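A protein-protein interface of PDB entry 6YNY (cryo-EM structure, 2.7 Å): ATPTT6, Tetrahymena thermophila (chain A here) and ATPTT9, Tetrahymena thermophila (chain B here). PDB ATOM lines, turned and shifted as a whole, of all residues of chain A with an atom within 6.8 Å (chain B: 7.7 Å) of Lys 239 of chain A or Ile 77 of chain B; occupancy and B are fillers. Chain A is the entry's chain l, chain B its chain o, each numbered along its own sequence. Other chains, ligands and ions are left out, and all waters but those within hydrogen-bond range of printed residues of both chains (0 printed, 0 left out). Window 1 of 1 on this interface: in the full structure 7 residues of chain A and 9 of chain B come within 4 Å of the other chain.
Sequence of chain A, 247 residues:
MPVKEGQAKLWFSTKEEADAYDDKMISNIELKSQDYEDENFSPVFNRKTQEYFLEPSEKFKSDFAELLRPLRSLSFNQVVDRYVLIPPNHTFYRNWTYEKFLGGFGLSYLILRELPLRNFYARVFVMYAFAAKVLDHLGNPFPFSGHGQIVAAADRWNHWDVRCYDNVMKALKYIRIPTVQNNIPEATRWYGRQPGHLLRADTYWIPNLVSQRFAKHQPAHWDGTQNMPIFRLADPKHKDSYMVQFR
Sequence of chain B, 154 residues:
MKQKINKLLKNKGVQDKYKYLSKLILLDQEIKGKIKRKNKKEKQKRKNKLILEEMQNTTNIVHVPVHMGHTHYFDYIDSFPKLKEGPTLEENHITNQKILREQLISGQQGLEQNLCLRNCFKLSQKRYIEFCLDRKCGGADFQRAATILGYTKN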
ATOM      1  N   ARG A 200      11.881 -29.790 -20.631  1.00  0.00           N
ATOM      2  CA  ARG A 200      11.682 -28.470 -21.217  1.00  0.00           C
ATOM      3  C   ARG A 200      11.160 -28.562 -22.643  1.00  0.00           C
ATOM      4  O   ARG A 200      10.400 -27.691 -23.080  1.00  0.00           O
ATOM      5  CB  ARG A 200      12.990 -27.685 -21.201  1.00  0.00           C
ATOM      6  CG  ARG A 200      13.374 -27.107 -19.864  1.00  0.00           C
ATOM      7  CD  ARG A 200      12.510 -25.929 -19.486  1.00  0.00           C
ATOM      8  NE  ARG A 200      12.587 -24.850 -20.464  1.00  0.00           N
ATOM      9  CZ  ARG A 200      13.489 -23.875 -20.442  1.00  0.00           C
ATOM     10  NH1 ARG A 200      13.471 -22.945 -21.382  1.00  0.00           N
ATOM     11  NH2 ARG A 200      14.406 -23.821 -19.487  1.00  0.00           N
ATOM     12  N   ASP A 235       5.441 -28.576 -11.356  1.00  0.00           N
ATOM     13  CA  ASP A 235       4.672 -27.838 -10.378  1.00  0.00           C
ATOM     14  C   ASP A 235       3.901 -26.749 -11.111  1.00  0.00           C
ATOM     15  O   ASP A 235       4.461 -26.080 -11.988  1.00  0.00           O
ATOM     16  CB  ASP A 235       5.562 -27.213  -9.298  1.00  0.00           C
ATOM     17  CG  ASP A 235       4.790 -26.832  -8.059  1.00  0.00           C
ATOM     18  OD1 ASP A 235       4.666 -27.682  -7.156  1.00  0.00           O
ATOM     19  OD2 ASP A 235       4.302 -25.686  -7.987  1.00  0.00           O
ATOM     20  N   PRO A 236       2.623 -26.552 -10.782  1.00  0.00           N
ATOM     21  CA  PRO A 236       1.844 -25.522 -11.486  1.00  0.00           C
ATOM     22  C   PRO A 236       2.398 -24.121 -11.329  1.00  0.00           C
ATOM     23  O   PRO A 236       2.186 -23.280 -12.209  1.00  0.00           O
ATOM     24  CB  PRO A 236       0.453 -25.639 -10.851  1.00  0.00           C
ATOM     25  CG  PRO A 236       0.423 -26.935 -10.196  1.00  0.00           C
ATOM     26  CD  PRO A 236       1.804 -27.284  -9.807  1.00  0.00           C
ATOM     27  N   LYS A 237       3.094 -23.842 -10.234  1.00  0.00           N
ATOM     28  CA  LYS A 237       3.581 -22.504  -9.938  1.00  0.00           C
ATOM     29  C   LYS A 237       4.968 -22.231 -10.499  1.00  0.00           C
ATOM     30  O   LYS A 237       5.480 -21.122 -10.331  1.00  0.00           O
ATOM     31  CB  LYS A 237       3.581 -22.280  -8.427  1.00  0.00           C
ATOM     32  CG  LYS A 237       2.269 -21.773  -7.873  1.00  0.00           C
ATOM     33  CD  LYS A 237       1.105 -22.669  -8.221  1.00  0.00           C
ATOM     34  CE  LYS A 237      -0.202 -22.046  -7.791  1.00  0.00           C
ATOM     35  NZ  LYS A 237      -1.378 -22.841  -8.218  1.00  0.00           N
ATOM     36  N   HIS A 238       5.581 -23.207 -11.156  1.00  0.00           N
ATOM     37  CA  HIS A 238       6.874 -22.996 -11.784  1.00  0.00           C
ATOM     38  C   HIS A 238       6.742 -22.028 -12.954  1.00  0.00           C
ATOM     39  O   HIS A 238       5.763 -22.066 -13.704  1.00  0.00           O
ATOM     40  CB  HIS A 238       7.440 -24.332 -12.253  1.00  0.00           C
ATOM     41  CG  HIS A 238       8.887 -24.283 -12.621  1.00  0.00           C
ATOM     42  ND1 HIS A 238       9.316 -24.159 -13.923  1.00  0.00           N
ATOM     43  CD2 HIS A 238      10.003 -24.350 -11.861  1.00  0.00           C
ATOM     44  CE1 HIS A 238      10.635 -24.146 -13.948  1.00  0.00           C
ATOM     45  NE2 HIS A 238      11.077 -24.260 -12.710  1.00  0.00           N
ATOM     46  N   LYS A 239       7.737 -21.152 -13.105  1.00  0.00           N
ATOM     47  CA  LYS A 239       7.676 -20.098 -14.108  1.00  0.00           C
ATOM     48  C   LYS A 239       7.748 -20.622 -15.535  1.00  0.00           C
ATOM     49  O   LYS A 239       7.467 -19.863 -16.466  1.00  0.00           O
ATOM     50  CB  LYS A 239       8.805 -19.095 -13.885  1.00  0.00           C
ATOM     51  CG  LYS A 239      10.187 -19.624 -14.193  1.00  0.00           C
ATOM     52  CD  LYS A 239      11.238 -18.561 -13.990  1.00  0.00           C
ATOM     53  CE  LYS A 239      12.621 -19.077 -14.312  1.00  0.00           C
ATOM     54  NZ  LYS A 239      12.746 -19.486 -15.727  1.00  0.00           N
ATOM     55  N   ASP A 240       8.119 -21.883 -15.728  1.00  0.00           N
ATOM     56  CA  ASP A 240       8.193 -22.486 -17.048  1.00  0.00           C
ATOM     57  C   ASP A 240       7.155 -23.578 -17.243  1.00  0.00           C
ATOM     58  O   ASP A 240       7.156 -24.235 -18.288  1.00  0.00           O
ATOM     59  CB  ASP A 240       9.592 -23.057 -17.293  1.00  0.00           C
ATOM     60  CG  ASP A 240      10.674 -22.000 -17.236  1.00  0.00           C
ATOM     61  OD1 ASP A 240      10.416 -20.855 -17.660  1.00  0.00           O
ATOM     62  OD2 ASP A 240      11.786 -22.315 -16.768  1.00  0.00           O
ATOM     63  N   SER A 241       6.267 -23.781 -16.271  1.00  0.00           N
ATOM     64  CA  SER A 241       5.253 -24.821 -16.341  1.00  0.00           C
ATOM     65  C   SER A 241       3.855 -24.284 -16.060  1.00  0.00           C
ATOM     66  O   SER A 241       2.916 -25.077 -15.932  1.00  0.00           O
ATOM     67  CB  SER A 241       5.579 -25.944 -15.357  1.00  0.00           C
ATOM     68  OG  SER A 241       6.896 -26.420 -15.554  1.00  0.00           O
ATOM     69  N   TYR A 242       3.691 -22.966 -15.966  1.00  0.00           N
ATOM     70  CA  TYR A 242       2.391 -22.397 -15.640  1.00  0.00           C
ATOM     71  C   TYR A 242       1.386 -22.565 -16.770  1.00  0.00           C
ATOM     72  O   TYR A 242       0.179 -22.500 -16.521  1.00  0.00           O
ATOM     73  CB  TYR A 242       2.544 -20.918 -15.287  1.00  0.00           C
ATOM     74  CG  TYR A 242       3.064 -20.051 -16.405  1.00  0.00           C
ATOM     75  CD1 TYR A 242       2.203 -19.494 -17.330  1.00  0.00           C
ATOM     76  CD2 TYR A 242       4.412 -19.777 -16.526  1.00  0.00           C
ATOM     77  CE1 TYR A 242       2.670 -18.699 -18.349  1.00  0.00           C
ATOM     78  CE2 TYR A 242       4.887 -18.981 -17.542  1.00  0.00           C
ATOM     79  CZ  TYR A 242       4.011 -18.444 -18.450  1.00  0.00           C
ATOM     80  OH  TYR A 242       4.482 -17.650 -19.466  1.00  0.00           O
ATOM     81  N   MET A 243       1.854 -22.777 -17.998  1.00  0.00           N
ATOM     82  CA  MET A 243       0.951 -23.030 -19.110  1.00  0.00           C
ATOM     83  C   MET A 243       0.361 -24.429 -19.060  1.00  0.00           C
ATOM     84  O   MET A 243      -0.631 -24.696 -19.744  1.00  0.00           O
ATOM     85  CB  MET A 243       1.688 -22.833 -20.429  1.00  0.00           C
ATOM     86  CG  MET A 243       2.816 -23.818 -20.661  1.00  0.00           C
ATOM     87  SD  MET A 243       4.086 -23.777 -19.396  1.00  0.00           S
ATOM     88  CE  MET A 243       4.787 -22.173 -19.718  1.00  0.00           C
ATOM     89  N   VAL B  62       4.033 -21.405   3.323  1.00  0.00           N
ATOM     90  CA  VAL B  62       5.407 -21.294   2.855  1.00  0.00           C
ATOM     91  C   VAL B  62       6.189 -20.447   3.845  1.00  0.00           C
ATOM     92  O   VAL B  62       5.664 -19.474   4.396  1.00  0.00           O
ATOM     93  CB  VAL B  62       5.481 -20.691   1.440  1.00  0.00           C
ATOM     94  CG1 VAL B  62       6.902 -20.700   0.944  1.00  0.00           C
ATOM     95  CG2 VAL B  62       4.598 -21.470   0.490  1.00  0.00           C
ATOM     96  N   PRO B  65      10.061 -16.157   1.317  1.00  0.00           N
ATOM     97  CA  PRO B  65       9.301 -15.248   0.456  1.00  0.00           C
ATOM     98  C   PRO B  65       9.179 -15.773  -0.966  1.00  0.00           C
ATOM     99  O   PRO B  65      10.072 -16.444  -1.486  1.00  0.00           O
ATOM    100  CB  PRO B  65      10.119 -13.954   0.499  1.00  0.00           C
ATOM    101  CG  PRO B  65      10.947 -14.061   1.706  1.00  0.00           C
ATOM    102  CD  PRO B  65      11.256 -15.504   1.868  1.00  0.00           C
ATOM    103  N   VAL B  66       8.052 -15.447  -1.595  1.00  0.00           N
ATOM    104  CA  VAL B  66       7.821 -15.742  -3.001  1.00  0.00           C
ATOM    105  C   VAL B  66       7.057 -14.578  -3.610  1.00  0.00           C
ATOM    106  O   VAL B  66       6.279 -13.899  -2.934  1.00  0.00           O
ATOM    107  CB  VAL B  66       7.038 -17.057  -3.212  1.00  0.00           C
ATOM    108  CG1 VAL B  66       7.753 -18.217  -2.576  1.00  0.00           C
ATOM    109  CG2 VAL B  66       5.642 -16.935  -2.659  1.00  0.00           C
ATOM    110  N   HIS B  67       7.288 -14.347  -4.898  1.00  0.00           N
ATOM    111  CA  HIS B  67       6.587 -13.318  -5.648  1.00  0.00           C
ATOM    112  C   HIS B  67       5.770 -13.973  -6.750  1.00  0.00           C
ATOM    113  O   HIS B  67       6.305 -14.750  -7.547  1.00  0.00           O
ATOM    114  CB  HIS B  67       7.558 -12.304  -6.243  1.00  0.00           C
ATOM    115  CG  HIS B  67       6.888 -11.095  -6.812  1.00  0.00           C
ATOM    116  ND1 HIS B  67       6.859 -10.826  -8.162  1.00  0.00           N
ATOM    117  CD2 HIS B  67       6.207 -10.090  -6.214  1.00  0.00           C
ATOM    118  CE1 HIS B  67       6.197  -9.703  -8.372  1.00  0.00           C
ATOM    119  NE2 HIS B  67       5.790  -9.237  -7.205  1.00  0.00           N
ATOM    120  N   MET B  68       4.481 -13.661  -6.788  1.00  0.00           N
ATOM    121  CA  MET B  68       3.559 -14.233  -7.754  1.00  0.00           C
ATOM    122  C   MET B  68       3.368 -13.292  -8.934  1.00  0.00           C
ATOM    123  O   MET B  68       3.384 -12.069  -8.788  1.00  0.00           O
ATOM    124  CB  MET B  68       2.208 -14.525  -7.105  1.00  0.00           C
ATOM    125  CG  MET B  68       2.193 -15.749  -6.214  1.00  0.00           C
ATOM    126  SD  MET B  68       2.257 -17.279  -7.156  1.00  0.00           S
ATOM    127  CE  MET B  68       1.922 -18.466  -5.867  1.00  0.00           C
ATOM    128  N   GLY B  69       3.188 -13.881 -10.114  1.00  0.00           N
ATOM    129  CA  GLY B  69       2.983 -13.090 -11.310  1.00  0.00           C
ATOM    130  C   GLY B  69       1.568 -12.542 -11.372  1.00  0.00           C
ATOM    131  O   GLY B  69       0.591 -13.240 -11.104  1.00  0.00           O
ATOM    132  N   ASP B  75      -1.241 -18.195 -13.092  1.00  0.00           N
ATOM    133  CA  ASP B  75      -0.926 -18.012 -11.677  1.00  0.00           C
ATOM    134  C   ASP B  75       0.317 -18.830 -11.367  1.00  0.00           C
ATOM    135  O   ASP B  75       0.272 -20.063 -11.404  1.00  0.00           O
ATOM    136  CB  ASP B  75      -2.093 -18.446 -10.793  1.00  0.00           C
ATOM    137  CG  ASP B  75      -1.807 -18.267  -9.321  1.00  0.00           C
ATOM    138  OD1 ASP B  75      -0.864 -17.522  -8.983  1.00  0.00           O
ATOM    139  OD2 ASP B  75      -2.519 -18.882  -8.499  1.00  0.00           O
ATOM    140  N   TYR B  76       1.418 -18.154 -11.058  1.00  0.00           N
ATOM    141  CA  TYR B  76       2.678 -18.844 -10.834  1.00  0.00           C
ATOM    142  C   TYR B  76       3.630 -17.930 -10.080  1.00  0.00           C
ATOM    143  O   TYR B  76       3.356 -16.748  -9.867  1.00  0.00           O
ATOM    144  CB  TYR B  76       3.305 -19.294 -12.152  1.00  0.00           C
ATOM    145  CG  TYR B  76       3.739 -18.156 -13.039  1.00  0.00           C
ATOM    146  CD1 TYR B  76       5.057 -17.744 -13.071  1.00  0.00           C
ATOM    147  CD2 TYR B  76       2.831 -17.490 -13.840  1.00  0.00           C
ATOM    148  CE1 TYR B  76       5.459 -16.710 -13.875  1.00  0.00           C
ATOM    149  CE2 TYR B  76       3.225 -16.455 -14.647  1.00  0.00           C
ATOM    150  CZ  TYR B  76       4.540 -16.068 -14.661  1.00  0.00           C
ATOM    151  OH  TYR B  76       4.937 -15.031 -15.467  1.00  0.00           O
ATOM    152  N   ILE B  77       4.761 -18.503  -9.689  1.00  0.00           N
ATOM    153  CA  ILE B  77       5.819 -17.791  -8.985  1.00  0.00           C
ATOM    154  C   ILE B  77       6.849 -17.370 -10.020  1.00  0.00           C
ATOM    155  O   ILE B  77       7.546 -18.211 -10.596  1.00  0.00           O
ATOM    156  CB  ILE B  77       6.447 -18.660  -7.890  1.00  0.00           C
ATOM    157  CG1 ILE B  77       5.410 -18.977  -6.815  1.00  0.00           C
ATOM    158  CG2 ILE B  77       7.643 -17.965  -7.289  1.00  0.00           C
ATOM    159  CD1 ILE B  77       5.814 -20.074  -5.883  1.00  0.00           C
ATOM    160  N   ASP B  78       6.949 -16.066 -10.259  1.00  0.00           N
ATOM    161  CA  ASP B  78       7.836 -15.550 -11.291  1.00  0.00           C
ATOM    162  C   ASP B  78       9.230 -15.228 -10.781  1.00  0.00           C
ATOM    163  O   ASP B  78      10.166 -15.165 -11.585  1.00  0.00           O
ATOM    164  CB  ASP B  78       7.231 -14.295 -11.925  1.00  0.00           C
ATOM    165  CG  ASP B  78       7.004 -13.187 -10.922  1.00  0.00           C
ATOM    166  OD1 ASP B  78       6.739 -13.497  -9.744  1.00  0.00           O
ATOM    167  OD2 ASP B  78       7.087 -12.005 -11.314  1.00  0.00           O
ATOM    168  N   SER B  79       9.401 -15.028  -9.478  1.00  0.00           N
ATOM    169  CA  SER B  79      10.693 -14.623  -8.953  1.00  0.00           C
ATOM    170  C   SER B  79      10.753 -14.917  -7.464  1.00  0.00           C
ATOM    171  O   SER B  79       9.727 -15.066  -6.798  1.00  0.00           O
ATOM    172  CB  SER B  79      10.947 -13.137  -9.205  1.00  0.00           C
ATOM    173  OG  SER B  79       9.950 -12.343  -8.591  1.00  0.00           O
ATOM    174  N   PHE B  80      11.979 -15.001  -6.956  1.00  0.00           N
ATOM    175  CA  PHE B  80      12.237 -15.116  -5.537  1.00  0.00           C
ATOM    176  C   PHE B  80      12.998 -13.886  -5.063  1.00  0.00           C
ATOM    177  O   PHE B  80      14.045 -13.556  -5.636  1.00  0.00           O
ATOM    178  CB  PHE B  80      13.042 -16.379  -5.222  1.00  0.00           C
ATOM    179  CG  PHE B  80      12.277 -17.646  -5.431  1.00  0.00           C
ATOM    180  CD1 PHE B  80      11.331 -18.053  -4.515  1.00  0.00           C
ATOM    181  CD2 PHE B  80      12.503 -18.430  -6.540  1.00  0.00           C
ATOM    182  CE1 PHE B  80      10.628 -19.212  -4.704  1.00  0.00           C
ATOM    183  CE2 PHE B  80      11.802 -19.590  -6.730  1.00  0.00           C
ATOM    184  CZ  PHE B  80      10.862 -19.982  -5.810  1.00  0.00           C
ATOM    185  N   PRO B  81      12.517 -13.180  -4.042  1.00  0.00           N
ATOM    186  CA  PRO B  81      13.205 -11.960  -3.605  1.00  0.00           C
ATOM    187  C   PRO B  81      14.646 -12.228  -3.191  1.00  0.00           C
ATOM    188  O   PRO B  81      14.939 -13.185  -2.473  1.00  0.00           O
ATOM    189  CB  PRO B  81      12.356 -11.482  -2.425  1.00  0.00           C
ATOM    190  CG  PRO B  81      11.026 -12.057  -2.665  1.00  0.00           C
ATOM    191  CD  PRO B  81      11.246 -13.370  -3.325  1.00  0.00           C
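Of the printed residues of chain B, Lys 237 of chain A touches Met 68 (3.9 Å), Asp 75 (3.99 Å), Tyr 76 (3.4 Å) and Ile 77 (2.8 Å).
Of chain B, only Tyr 76 and Ile 77 come within 4 Å of Lys 239 of chain A.
Ser 241 of chain A touches none of the printed residues of chain B.
Gly 69 of chain B touches none of the printed residues of chain A.
Of the printed residues of chain A, Asp 75 of chain B touches Pro 236 (3.8 Å) and Lys 237 (3.99 Å).
Printed residues of chain A within 4 Å of Tyr 76 of chain B: Lys 237, Lys 239 and Tyr 242.
Of chain A, only Lys 237 (2.8 Å) and Lys 239 (3.6 Å) come within 4 Å of Ile 77 of chain B.
The nearest residue of chain A that does not touch Ile 77 of chain B is His 238 of chain A (4.6 Å).
Hydrophobic or aromatic side chains of chain B that line the printed part of chain A: Met 68, Tyr 76 and Ile 77.
Among the printed residues, no Asp or Glu carboxylate lies within 4 Å of a Lys or Arg side-chain nitrogen of the other chain.
Pro 236 of chain A touches Asp 75 of chain B.
Met 68 of chain B touches Lys 237 of chain A.
CE of Lys 237 of chain A touches OD2 of Asp 75 of chain B (3.99 Å).
CB of Tyr 76 of chain B touches O of Lys 237 of chain A, 3.4 Å away.
Lys 239 of chain A touches Tyr 76 of chain B.
CB of Lys 239 of chain A touches O of Ile 77 of chain B (3.6 Å).
CB of Tyr 242 of chain A touches CB of Tyr 76 of chain B (3.6 Å).
The backbone NH (N) of Lys 237 of chain A sits close to the side-chain carboxylate (OD2) of Asp 235 of chain A, 3.1 Å away.
The side-chain amino group (NZ) of Lys 239 of chain A lies within salt-bridge range of the side-chain carboxylate (OD2) of Asp 240 of chain A (3.2 Å).
N of Ile 77 of chain B sits close to SD of Met 68 of chain B (3.8 Å).
N of Gly 69 of chain B lies within hydrogen-bond range of O of Tyr 76 of chain B (2.9 Å).
The backbone carbonyl oxygen of Lys 237 of chain A is in hydrogen-bond range of the backbone NH of Ile 77 of chain B (2.8 Å).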
